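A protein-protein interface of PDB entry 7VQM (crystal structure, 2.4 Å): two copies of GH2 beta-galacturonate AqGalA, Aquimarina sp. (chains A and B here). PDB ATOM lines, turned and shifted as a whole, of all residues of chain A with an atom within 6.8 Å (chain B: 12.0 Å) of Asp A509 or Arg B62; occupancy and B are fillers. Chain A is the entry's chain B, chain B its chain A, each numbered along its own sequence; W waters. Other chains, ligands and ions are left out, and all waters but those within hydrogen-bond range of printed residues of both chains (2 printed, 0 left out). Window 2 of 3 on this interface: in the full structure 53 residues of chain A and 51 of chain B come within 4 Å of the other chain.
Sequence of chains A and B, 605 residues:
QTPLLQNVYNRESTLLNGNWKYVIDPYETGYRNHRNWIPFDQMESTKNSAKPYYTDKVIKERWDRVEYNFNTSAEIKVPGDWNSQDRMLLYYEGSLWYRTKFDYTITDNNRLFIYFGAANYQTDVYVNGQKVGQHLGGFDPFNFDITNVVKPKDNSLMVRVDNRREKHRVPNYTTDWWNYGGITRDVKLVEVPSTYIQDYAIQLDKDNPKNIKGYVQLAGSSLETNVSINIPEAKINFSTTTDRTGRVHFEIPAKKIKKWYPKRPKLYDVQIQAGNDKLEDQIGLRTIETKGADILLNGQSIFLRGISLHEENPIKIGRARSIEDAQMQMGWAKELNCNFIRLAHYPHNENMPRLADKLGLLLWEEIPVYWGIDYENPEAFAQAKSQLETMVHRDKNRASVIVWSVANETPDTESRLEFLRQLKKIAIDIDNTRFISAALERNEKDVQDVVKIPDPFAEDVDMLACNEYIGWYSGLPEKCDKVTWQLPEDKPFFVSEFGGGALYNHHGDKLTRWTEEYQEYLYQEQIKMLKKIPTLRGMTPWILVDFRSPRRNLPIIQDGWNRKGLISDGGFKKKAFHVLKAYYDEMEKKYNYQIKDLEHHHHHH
Arg B62 touches Leu A511. Leu A511 touches Trp B63. Arg A513 touches Arg B65.
OD2 of Asp A509 lies within salt-bridge range of NH2 of Arg B62, at 3.0 Å. The guanidinium group (NE) of Arg B62 lies close to the side-chain hydroxyl (OG1) of Thr A512 (3.3 Å). The backbone NH (N) of Arg A513 lies within hydrogen-bond range of the backbone carbonyl oxygen (O) of Arg B62, 2.9 Å away. The backbone carbonyl oxygen (O) of Trp B63 sits at hydrogen-bond distance from the guanidinium group (NE) of Arg A513 (2.9 Å). The guanidinium group (NE) of Arg A513 lies within hydrogen-bond range of the backbone carbonyl oxygen (O) of Asp B64, 3.3 Å away.
No position is printed for both chains. Of the 8 pairs that touch across the chains among the printed residues, none has its exchanged pair printed and touching as well.
N of Glu B61 lies within hydrogen-bond range of OD2 of Asp B64, 2.9 Å away. The guanidinium group of Arg B65 is in salt-bridge range of the side-chain carboxylate of Glu B67, 2.7 Å away. The side-chain carboxylate (OD2) of Asp A509 lies close to the backbone NH (N) of Leu A511 (3.4 Å). OG1 of Thr A515 sits at hydrogen-bond distance from O of Asp A509 (3.4 Å). The backbone carbonyl oxygen of Thr A512 sits at hydrogen-bond distance from the side-chain hydroxyl of Thr A515 (2.6 Å). The guanidinium group of Arg A513 sits at hydrogen-bond distance from the side-chain hydroxyl of Tyr A518, at 3.4 Å.
Water W2 bridges the guanidinium group (NE) of Arg B65 (2.7 Å) and the guanidinium group (NH2) of Arg A513 (3.5 Å). Water W1 bridges N of Val B66 (2.8 Å) and NE1 of Trp A514 (3.1 Å).
Asp A509 touches just one residue of chain B: Arg B62 (3.0 Å). Of chain A, only Asp A509 (3.0 Å), Leu A511 (3.8 Å), Thr A512 (3.2 Å) and Arg A513 (2.9 Å) come within 4 Å of Arg B62. Gly A508 touches none of the printed residues of chain B. No residue of chain B comes within 4 Å of Lys A510. Arg A513 touches just these residues of chain B: Arg B62, Trp B63, Asp B64 and Arg B65. No residue of chain B comes within 4 Å of Thr A515. No residue of chain B comes within 4 Å of Glu A517. Printed residues of chain A within 4 Å of Trp B63: Leu A511 and Arg A513. Of the printed residues of chain A, Arg B65 touches Arg A513 (3.5 Å). Of the printed residues of chain A, Asp B64 touches Arg A513. Glu B61 touches none of the printed residues of chain A. The nearest residue of chain B that does not touch Asp A509 is Trp B63 (6.6 Å). The nearest printed residue of chain A that does not touch Asp B64 is Trp A514 (4.9 Å).
Printed residues of chain B that touch a printed residue of chain A: Arg B62, Trp B63, Asp B64 and Arg B65. Hydrophobic or aromatic side chains of chain B that line the printed part of chain A: Trp B63. Of the 11 printed residues of chain A, 4 touch a printed residue of chain B. Among the printed residues, 8 pairs touch across the chains. Among the printed residues, Asp or Glu carboxylates within 4 Å of a Lys or Arg side-chain nitrogen of the other chain: Asp A509 with Arg B62.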
ATOM      1  N   HIS A 507     -18.507 -26.611  -6.279  1.00  0.00           N
ATOM      2  CA  HIS A 507     -18.510 -27.428  -5.043  1.00  0.00           C
ATOM      3  C   HIS A 507     -18.141 -26.566  -3.838  1.00  0.00           C
ATOM      4  O   HIS A 507     -17.457 -25.530  -4.001  1.00  0.00           O
ATOM      5  CB  HIS A 507     -17.617 -28.662  -5.178  1.00  0.00           C
ATOM      6  CG  HIS A 507     -18.134 -29.660  -6.153  1.00  0.00           C
ATOM      7  ND1 HIS A 507     -19.075 -30.604  -5.810  1.00  0.00           N
ATOM      8  CD2 HIS A 507     -17.855 -29.852  -7.458  1.00  0.00           C
ATOM      9  CE1 HIS A 507     -19.337 -31.349  -6.864  1.00  0.00           C
ATOM     10  NE2 HIS A 507     -18.604 -30.909  -7.896  1.00  0.00           N
ATOM     11  N   GLY A 508     -18.632 -26.970  -2.671  1.00  0.00           N
ATOM     12  CA  GLY A 508     -18.119 -26.454  -1.394  1.00  0.00           C
ATOM     13  C   GLY A 508     -18.806 -27.101  -0.224  1.00  0.00           C
ATOM     14  O   GLY A 508     -19.309 -28.236  -0.359  1.00  0.00           O
ATOM     15  N   ASP A 509     -18.826 -26.370   0.878  1.00  0.00           N
ATOM     16  CA  ASP A 509     -19.528 -26.707   2.139  1.00  0.00           C
ATOM     17  C   ASP A 509     -21.046 -26.651   1.888  1.00  0.00           C
ATOM     18  O   ASP A 509     -21.473 -25.862   1.035  1.00  0.00           O
ATOM     19  CB  ASP A 509     -18.978 -25.752   3.198  1.00  0.00           C
ATOM     20  CG  ASP A 509     -19.841 -25.592   4.417  1.00  0.00           C
ATOM     21  OD1 ASP A 509     -19.925 -26.573   5.212  1.00  0.00           O
ATOM     22  OD2 ASP A 509     -20.437 -24.497   4.532  1.00  0.00           O
ATOM     23  N   LYS A 510     -21.840 -27.448   2.607  1.00  0.00           N
ATOM     24  CA  LYS A 510     -23.305 -27.620   2.359  1.00  0.00           C
ATOM     25  C   LYS A 510     -24.079 -26.327   2.639  1.00  0.00           C
ATOM     26  O   LYS A 510     -25.280 -26.266   2.270  1.00  0.00           O
ATOM     27  CB  LYS A 510     -23.897 -28.730   3.235  1.00  0.00           C
ATOM     28  CG  LYS A 510     -23.888 -28.429   4.728  1.00  0.00           C
ATOM     29  CD  LYS A 510     -24.793 -29.321   5.547  1.00  0.00           C
ATOM     30  CE  LYS A 510     -24.064 -30.463   6.210  1.00  0.00           C
ATOM     31  NZ  LYS A 510     -25.022 -31.336   6.923  1.00  0.00           N
ATOM     32  N   LEU A 511     -23.472 -25.359   3.330  1.00  0.00           N
ATOM     33  CA  LEU A 511     -24.122 -24.057   3.608  1.00  0.00           C
ATOM     34  C   LEU A 511     -23.736 -23.027   2.552  1.00  0.00           C
ATOM     35  O   LEU A 511     -24.270 -21.913   2.641  1.00  0.00           O
ATOM     36  CB  LEU A 511     -23.719 -23.566   4.997  1.00  0.00           C
ATOM     37  CG  LEU A 511     -24.474 -24.195   6.163  1.00  0.00           C
ATOM     38  CD1 LEU A 511     -23.880 -23.708   7.479  1.00  0.00           C
ATOM     39  CD2 LEU A 511     -25.962 -23.873   6.092  1.00  0.00           C
ATOM     40  N   THR A 512     -22.841 -23.354   1.613  1.00  0.00           N
ATOM     41  CA  THR A 512     -22.440 -22.409   0.534  1.00  0.00           C
ATOM     42  C   THR A 512     -23.488 -22.489  -0.579  1.00  0.00           C
ATOM     43  O   THR A 512     -23.513 -23.495  -1.300  1.00  0.00           O
ATOM     44  CB  THR A 512     -21.011 -22.661   0.047  1.00  0.00           C
ATOM     45  OG1 THR A 512     -20.097 -22.293   1.082  1.00  0.00           O
ATOM     46  CG2 THR A 512     -20.656 -21.855  -1.185  1.00  0.00           C
ATOM     47  N   ARG A 513     -24.341 -21.473  -0.699  1.00  0.00           N
ATOM     48  CA  ARG A 513     -25.480 -21.494  -1.652  1.00  0.00           C
ATOM     49  C   ARG A 513     -24.960 -21.582  -3.093  1.00  0.00           C
ATOM     50  O   ARG A 513     -23.929 -20.970  -3.406  1.00  0.00           O
ATOM     51  CB  ARG A 513     -26.383 -20.277  -1.464  1.00  0.00           C
ATOM     52  CG  ARG A 513     -27.792 -20.534  -1.970  1.00  0.00           C
ATOM     53  CD  ARG A 513     -28.669 -19.315  -1.866  1.00  0.00           C
ATOM     54  NE  ARG A 513     -29.222 -19.056  -0.547  1.00  0.00           N
ATOM     55  CZ  ARG A 513     -30.399 -19.467  -0.120  1.00  0.00           C
ATOM     56  NH1 ARG A 513     -31.168 -20.227  -0.890  1.00  0.00           N
ATOM     57  NH2 ARG A 513     -30.808 -19.102   1.080  1.00  0.00           N
ATOM     58  N   TRP A 514     -25.647 -22.386  -3.903  1.00  0.00           N
ATOM     59  CA  TRP A 514     -25.424 -22.630  -5.348  1.00  0.00           C
ATOM     60  C   TRP A 514     -24.448 -23.779  -5.549  1.00  0.00           C
ATOM     61  O   TRP A 514     -24.316 -24.208  -6.725  1.00  0.00           O
ATOM     62  CB  TRP A 514     -24.936 -21.383  -6.096  1.00  0.00           C
ATOM     63  CG  TRP A 514     -25.829 -20.202  -5.925  1.00  0.00           C
ATOM     64  CD1 TRP A 514     -25.599 -19.084  -5.177  1.00  0.00           C
ATOM     65  CD2 TRP A 514     -27.104 -20.025  -6.542  1.00  0.00           C
ATOM     66  NE1 TRP A 514     -26.653 -18.226  -5.285  1.00  0.00           N
ATOM     67  CE2 TRP A 514     -27.586 -18.770  -6.123  1.00  0.00           C
ATOM     68  CE3 TRP A 514     -27.871 -20.794  -7.421  1.00  0.00           C
ATOM     69  CZ2 TRP A 514     -28.815 -18.276  -6.545  1.00  0.00           C
ATOM     70  CZ3 TRP A 514     -29.089 -20.300  -7.836  1.00  0.00           C
ATOM     71  CH2 TRP A 514     -29.549 -19.058  -7.405  1.00  0.00           C
ATOM     72  N   THR A 515     -23.777 -24.240  -4.487  1.00  0.00           N
ATOM     73  CA  THR A 515     -22.926 -25.463  -4.581  1.00  0.00           C
ATOM     74  C   THR A 515     -23.853 -26.666  -4.701  1.00  0.00           C
ATOM     75  O   THR A 515     -25.006 -26.591  -4.236  1.00  0.00           O
ATOM     76  CB  THR A 515     -21.934 -25.672  -3.425  1.00  0.00           C
ATOM     77  OG1 THR A 515     -22.589 -25.775  -2.161  1.00  0.00           O
ATOM     78  CG2 THR A 515     -20.910 -24.567  -3.370  1.00  0.00           C
ATOM     79  N   GLU A 517     -23.437 -29.234  -3.011  1.00  0.00           N
ATOM     80  CA  GLU A 517     -23.497 -29.763  -1.619  1.00  0.00           C
ATOM     81  C   GLU A 517     -24.688 -29.134  -0.897  1.00  0.00           C
ATOM     82  O   GLU A 517     -25.299 -29.833  -0.063  1.00  0.00           O
ATOM     83  CB  GLU A 517     -22.199 -29.516  -0.845  1.00  0.00           C
ATOM     84  CG  GLU A 517     -21.076 -30.471  -1.220  1.00  0.00           C
ATOM     85  CD  GLU A 517     -20.498 -30.227  -2.605  1.00  0.00           C
ATOM     86  OE1 GLU A 517     -20.706 -29.115  -3.138  1.00  0.00           O
ATOM     87  OE2 GLU A 517     -19.825 -31.132  -3.144  1.00  0.00           O
ATOM     88  N   TYR A 518     -25.004 -27.870  -1.195  1.00  0.00           N
ATOM     89  CA  TYR A 518     -26.176 -27.186  -0.599  1.00  0.00           C
ATOM     90  C   TYR A 518     -27.437 -27.846  -1.153  1.00  0.00           C
ATOM     91  O   TYR A 518     -28.320 -28.194  -0.348  1.00  0.00           O
ATOM     92  CB  TYR A 518     -26.129 -25.678  -0.839  1.00  0.00           C
ATOM     93  CG  TYR A 518     -27.249 -24.883  -0.216  1.00  0.00           C
ATOM     94  CD1 TYR A 518     -28.564 -25.104  -0.588  1.00  0.00           C
ATOM     95  CD2 TYR A 518     -26.995 -23.868   0.699  1.00  0.00           C
ATOM     96  CE1 TYR A 518     -29.599 -24.352  -0.060  1.00  0.00           C
ATOM     97  CE2 TYR A 518     -28.021 -23.109   1.241  1.00  0.00           C
ATOM     98  CZ  TYR A 518     -29.332 -23.355   0.863  1.00  0.00           C
ATOM     99  OH  TYR A 518     -30.387 -22.622   1.344  1.00  0.00           O
ATOM    100  N   VAL B  58     -24.803  -6.962  -2.659  1.00  0.00           N
ATOM    101  CA  VAL B  58     -24.047  -8.249  -2.729  1.00  0.00           C
ATOM    102  C   VAL B  58     -24.365  -9.047  -1.446  1.00  0.00           C
ATOM    103  O   VAL B  58     -24.816  -8.457  -0.441  1.00  0.00           O
ATOM    104  CB  VAL B  58     -22.530  -8.021  -2.932  1.00  0.00           C
ATOM    105  CG1 VAL B  58     -22.192  -7.438  -4.302  1.00  0.00           C
ATOM    106  CG2 VAL B  58     -21.939  -7.138  -1.843  1.00  0.00           C
ATOM    107  N   ILE B  59     -24.152 -10.361  -1.474  1.00  0.00           N
ATOM    108  CA  ILE B  59     -24.284 -11.254  -0.284  1.00  0.00           C
ATOM    109  C   ILE B  59     -23.323 -10.791   0.811  1.00  0.00           C
ATOM    110  O   ILE B  59     -22.244 -10.315   0.454  1.00  0.00           O
ATOM    111  CB  ILE B  59     -24.014 -12.720  -0.678  1.00  0.00           C
ATOM    112  CG1 ILE B  59     -22.614 -12.905  -1.286  1.00  0.00           C
ATOM    113  CG2 ILE B  59     -25.136 -13.230  -1.581  1.00  0.00           C
ATOM    114  CD1 ILE B  59     -22.298 -14.315  -1.746  1.00  0.00           C
ATOM    115  N   LYS B  60     -23.697 -10.950   2.083  1.00  0.00           N
ATOM    116  CA  LYS B  60     -22.788 -10.745   3.257  1.00  0.00           C
ATOM    117  C   LYS B  60     -22.227 -12.091   3.747  1.00  0.00           C
ATOM    118  O   LYS B  60     -21.099 -12.120   4.221  1.00  0.00           O
ATOM    119  CB  LYS B  60     -23.519 -10.042   4.403  1.00  0.00           C
ATOM    120  CG  LYS B  60     -24.111  -8.689   4.034  1.00  0.00           C
ATOM    121  CD  LYS B  60     -25.518  -8.442   4.583  1.00  0.00           C
ATOM    122  CE  LYS B  60     -26.025  -7.030   4.361  1.00  0.00           C
ATOM    123  NZ  LYS B  60     -25.055  -6.020   4.843  1.00  0.00           N
ATOM    124  N   GLU B  61     -23.009 -13.160   3.651  1.00  0.00           N
ATOM    125  CA  GLU B  61     -22.561 -14.536   3.955  1.00  0.00           C
ATOM    126  C   GLU B  61     -22.853 -15.436   2.754  1.00  0.00           C
ATOM    127  O   GLU B  61     -23.706 -15.074   1.910  1.00  0.00           O
ATOM    128  CB  GLU B  61     -23.284 -15.077   5.188  1.00  0.00           C
ATOM    129  CG  GLU B  61     -23.328 -14.100   6.346  1.00  0.00           C
ATOM    130  CD  GLU B  61     -22.087 -14.087   7.218  1.00  0.00           C
ATOM    131  OE1 GLU B  61     -21.009 -14.448   6.724  1.00  0.00           O
ATOM    132  OE2 GLU B  61     -22.220 -13.714   8.401  1.00  0.00           O
ATOM    133  N   ARG B  62     -22.230 -16.608   2.743  1.00  0.00           N
ATOM    134  CA  ARG B  62     -22.221 -17.533   1.587  1.00  0.00           C
ATOM    135  C   ARG B  62     -23.556 -18.293   1.476  1.00  0.00           C
ATOM    136  O   ARG B  62     -23.791 -18.886   0.405  1.00  0.00           O
ATOM    137  CB  ARG B  62     -20.994 -18.435   1.717  1.00  0.00           C
ATOM    138  CG  ARG B  62     -21.110 -19.474   2.821  1.00  0.00           C
ATOM    139  CD  ARG B  62     -19.731 -19.921   3.255  1.00  0.00           C
ATOM    140  NE  ARG B  62     -19.737 -21.075   4.141  1.00  0.00           N
ATOM    141  CZ  ARG B  62     -19.555 -21.031   5.463  1.00  0.00           C
ATOM    142  NH1 ARG B  62     -19.397 -19.873   6.090  1.00  0.00           N
ATOM    143  NH2 ARG B  62     -19.528 -22.159   6.157  1.00  0.00           N
ATOM    144  N   TRP B  63     -24.423 -18.236   2.494  1.00  0.00           N
ATOM    145  CA  TRP B  63     -25.761 -18.899   2.500  1.00  0.00           C
ATOM    146  C   TRP B  63     -26.868 -17.933   2.054  1.00  0.00           C
ATOM    147  O   TRP B  63     -28.032 -18.379   1.955  1.00  0.00           O
ATOM    148  CB  TRP B  63     -26.104 -19.476   3.885  1.00  0.00           C
ATOM    149  CG  TRP B  63     -26.046 -18.479   5.002  1.00  0.00           C
ATOM    150  CD1 TRP B  63     -26.974 -17.539   5.347  1.00  0.00           C
ATOM    151  CD2 TRP B  63     -24.951 -18.304   5.904  1.00  0.00           C
ATOM    152  NE1 TRP B  63     -26.528 -16.793   6.404  1.00  0.00           N
ATOM    153  CE2 TRP B  63     -25.291 -17.247   6.773  1.00  0.00           C
ATOM    154  CE3 TRP B  63     -23.724 -18.944   6.053  1.00  0.00           C
ATOM    155  CZ2 TRP B  63     -24.432 -16.808   7.776  1.00  0.00           C
ATOM    156  CZ3 TRP B  63     -22.886 -18.528   7.062  1.00  0.00           C
ATOM    157  CH2 TRP B  63     -23.232 -17.470   7.898  1.00  0.00           C
ATOM    158  N   ASP B  64     -26.556 -16.651   1.868  1.00  0.00           N
ATOM    159  CA  ASP B  64     -27.536 -15.650   1.365  1.00  0.00           C
ATOM    160  C   ASP B  64     -27.816 -15.923  -0.108  1.00  0.00           C
ATOM    161  O   ASP B  64     -26.994 -16.589  -0.728  1.00  0.00           O
ATOM    162  CB  ASP B  64     -27.014 -14.223   1.479  1.00  0.00           C
ATOM    163  CG  ASP B  64     -26.847 -13.772   2.904  1.00  0.00           C
ATOM    164  OD1 ASP B  64     -27.672 -14.182   3.737  1.00  0.00           O
ATOM    165  OD2 ASP B  64     -25.871 -13.037   3.157  1.00  0.00           O
ATOM    166  N   ARG B  65     -28.900 -15.348  -0.631  1.00  0.00           N
ATOM    167  CA  ARG B  65     -29.325 -15.473  -2.053  1.00  0.00           C
ATOM    168  C   ARG B  65     -29.591 -14.092  -2.658  1.00  0.00           C
ATOM    169  O   ARG B  65     -30.471 -13.393  -2.151  1.00  0.00           O
ATOM    170  CB  ARG B  65     -30.598 -16.313  -2.151  1.00  0.00           C
ATOM    171  CG  ARG B  65     -31.015 -16.690  -3.565  1.00  0.00           C
ATOM    172  CD  ARG B  65     -32.259 -17.553  -3.501  1.00  0.00           C
ATOM    173  NE  ARG B  65     -33.275 -16.865  -2.722  1.00  0.00           N
ATOM    174  CZ  ARG B  65     -34.106 -15.953  -3.197  1.00  0.00           C
ATOM    175  NH1 ARG B  65     -34.096 -15.643  -4.481  1.00  0.00           N
ATOM    176  NH2 ARG B  65     -34.969 -15.370  -2.392  1.00  0.00           N
ATOM    177  N   VAL B  66     -28.866 -13.729  -3.716  1.00  0.00           N
ATOM    178  CA  VAL B  66     -29.140 -12.518  -4.541  1.00  0.00           C
ATOM    179  C   VAL B  66     -28.989 -12.930  -6.001  1.00  0.00           C
ATOM    180  O   VAL B  66     -27.888 -13.369  -6.336  1.00  0.00           O
ATOM    181  CB  VAL B  66     -28.190 -11.367  -4.180  1.00  0.00           C
ATOM    182  CG1 VAL B  66     -28.600 -10.077  -4.861  1.00  0.00           C
ATOM    183  CG2 VAL B  66     -28.103 -11.167  -2.677  1.00  0.00           C
ATOM    184  N   GLU B  67     -30.045 -12.789  -6.810  1.00  0.00           N
ATOM    185  CA  GLU B  67     -30.129 -13.393  -8.170  1.00  0.00           C
ATOM    186  C   GLU B  67     -29.703 -12.344  -9.197  1.00  0.00           C
ATOM    187  O   GLU B  67     -30.220 -12.350 -10.318  1.00  0.00           O
ATOM    188  CB  GLU B  67     -31.515 -14.005  -8.375  1.00  0.00           C
ATOM    189  CG  GLU B  67     -31.784 -15.147  -7.410  1.00  0.00           C
ATOM    190  CD  GLU B  67     -32.814 -16.195  -7.791  1.00  0.00           C
ATOM    191  OE1 GLU B  67     -33.022 -16.437  -8.997  1.00  0.00           O
ATOM    192  OE2 GLU B  67     -33.407 -16.783  -6.862  1.00  0.00           O
ATOM    193  N   ASN B  69     -25.872  -9.502  -9.769  1.00  0.00           N
ATOM    194  CA  ASN B  69     -24.567  -9.000  -9.278  1.00  0.00           C
ATOM    195  C   ASN B  69     -23.938  -8.158 -10.383  1.00  0.00           C
ATOM    196  O   ASN B  69     -23.288  -8.724 -11.260  1.00  0.00           O
ATOM    197  CB  ASN B  69     -23.640 -10.132  -8.848  1.00  0.00           C
ATOM    198  CG  ASN B  69     -22.391  -9.599  -8.193  1.00  0.00           C
ATOM    199  OD1 ASN B  69     -21.996  -8.458  -8.431  1.00  0.00           O
ATOM    200  ND2 ASN B  69     -21.771 -10.417  -7.361  1.00  0.00           N
HETATM  201  O   HOH W   1     -26.635 -15.277  -4.197  1.00  0.00           O
HETATM  202  O   HOH W   2     -33.486 -17.178  -0.002  1.00  0.00           O
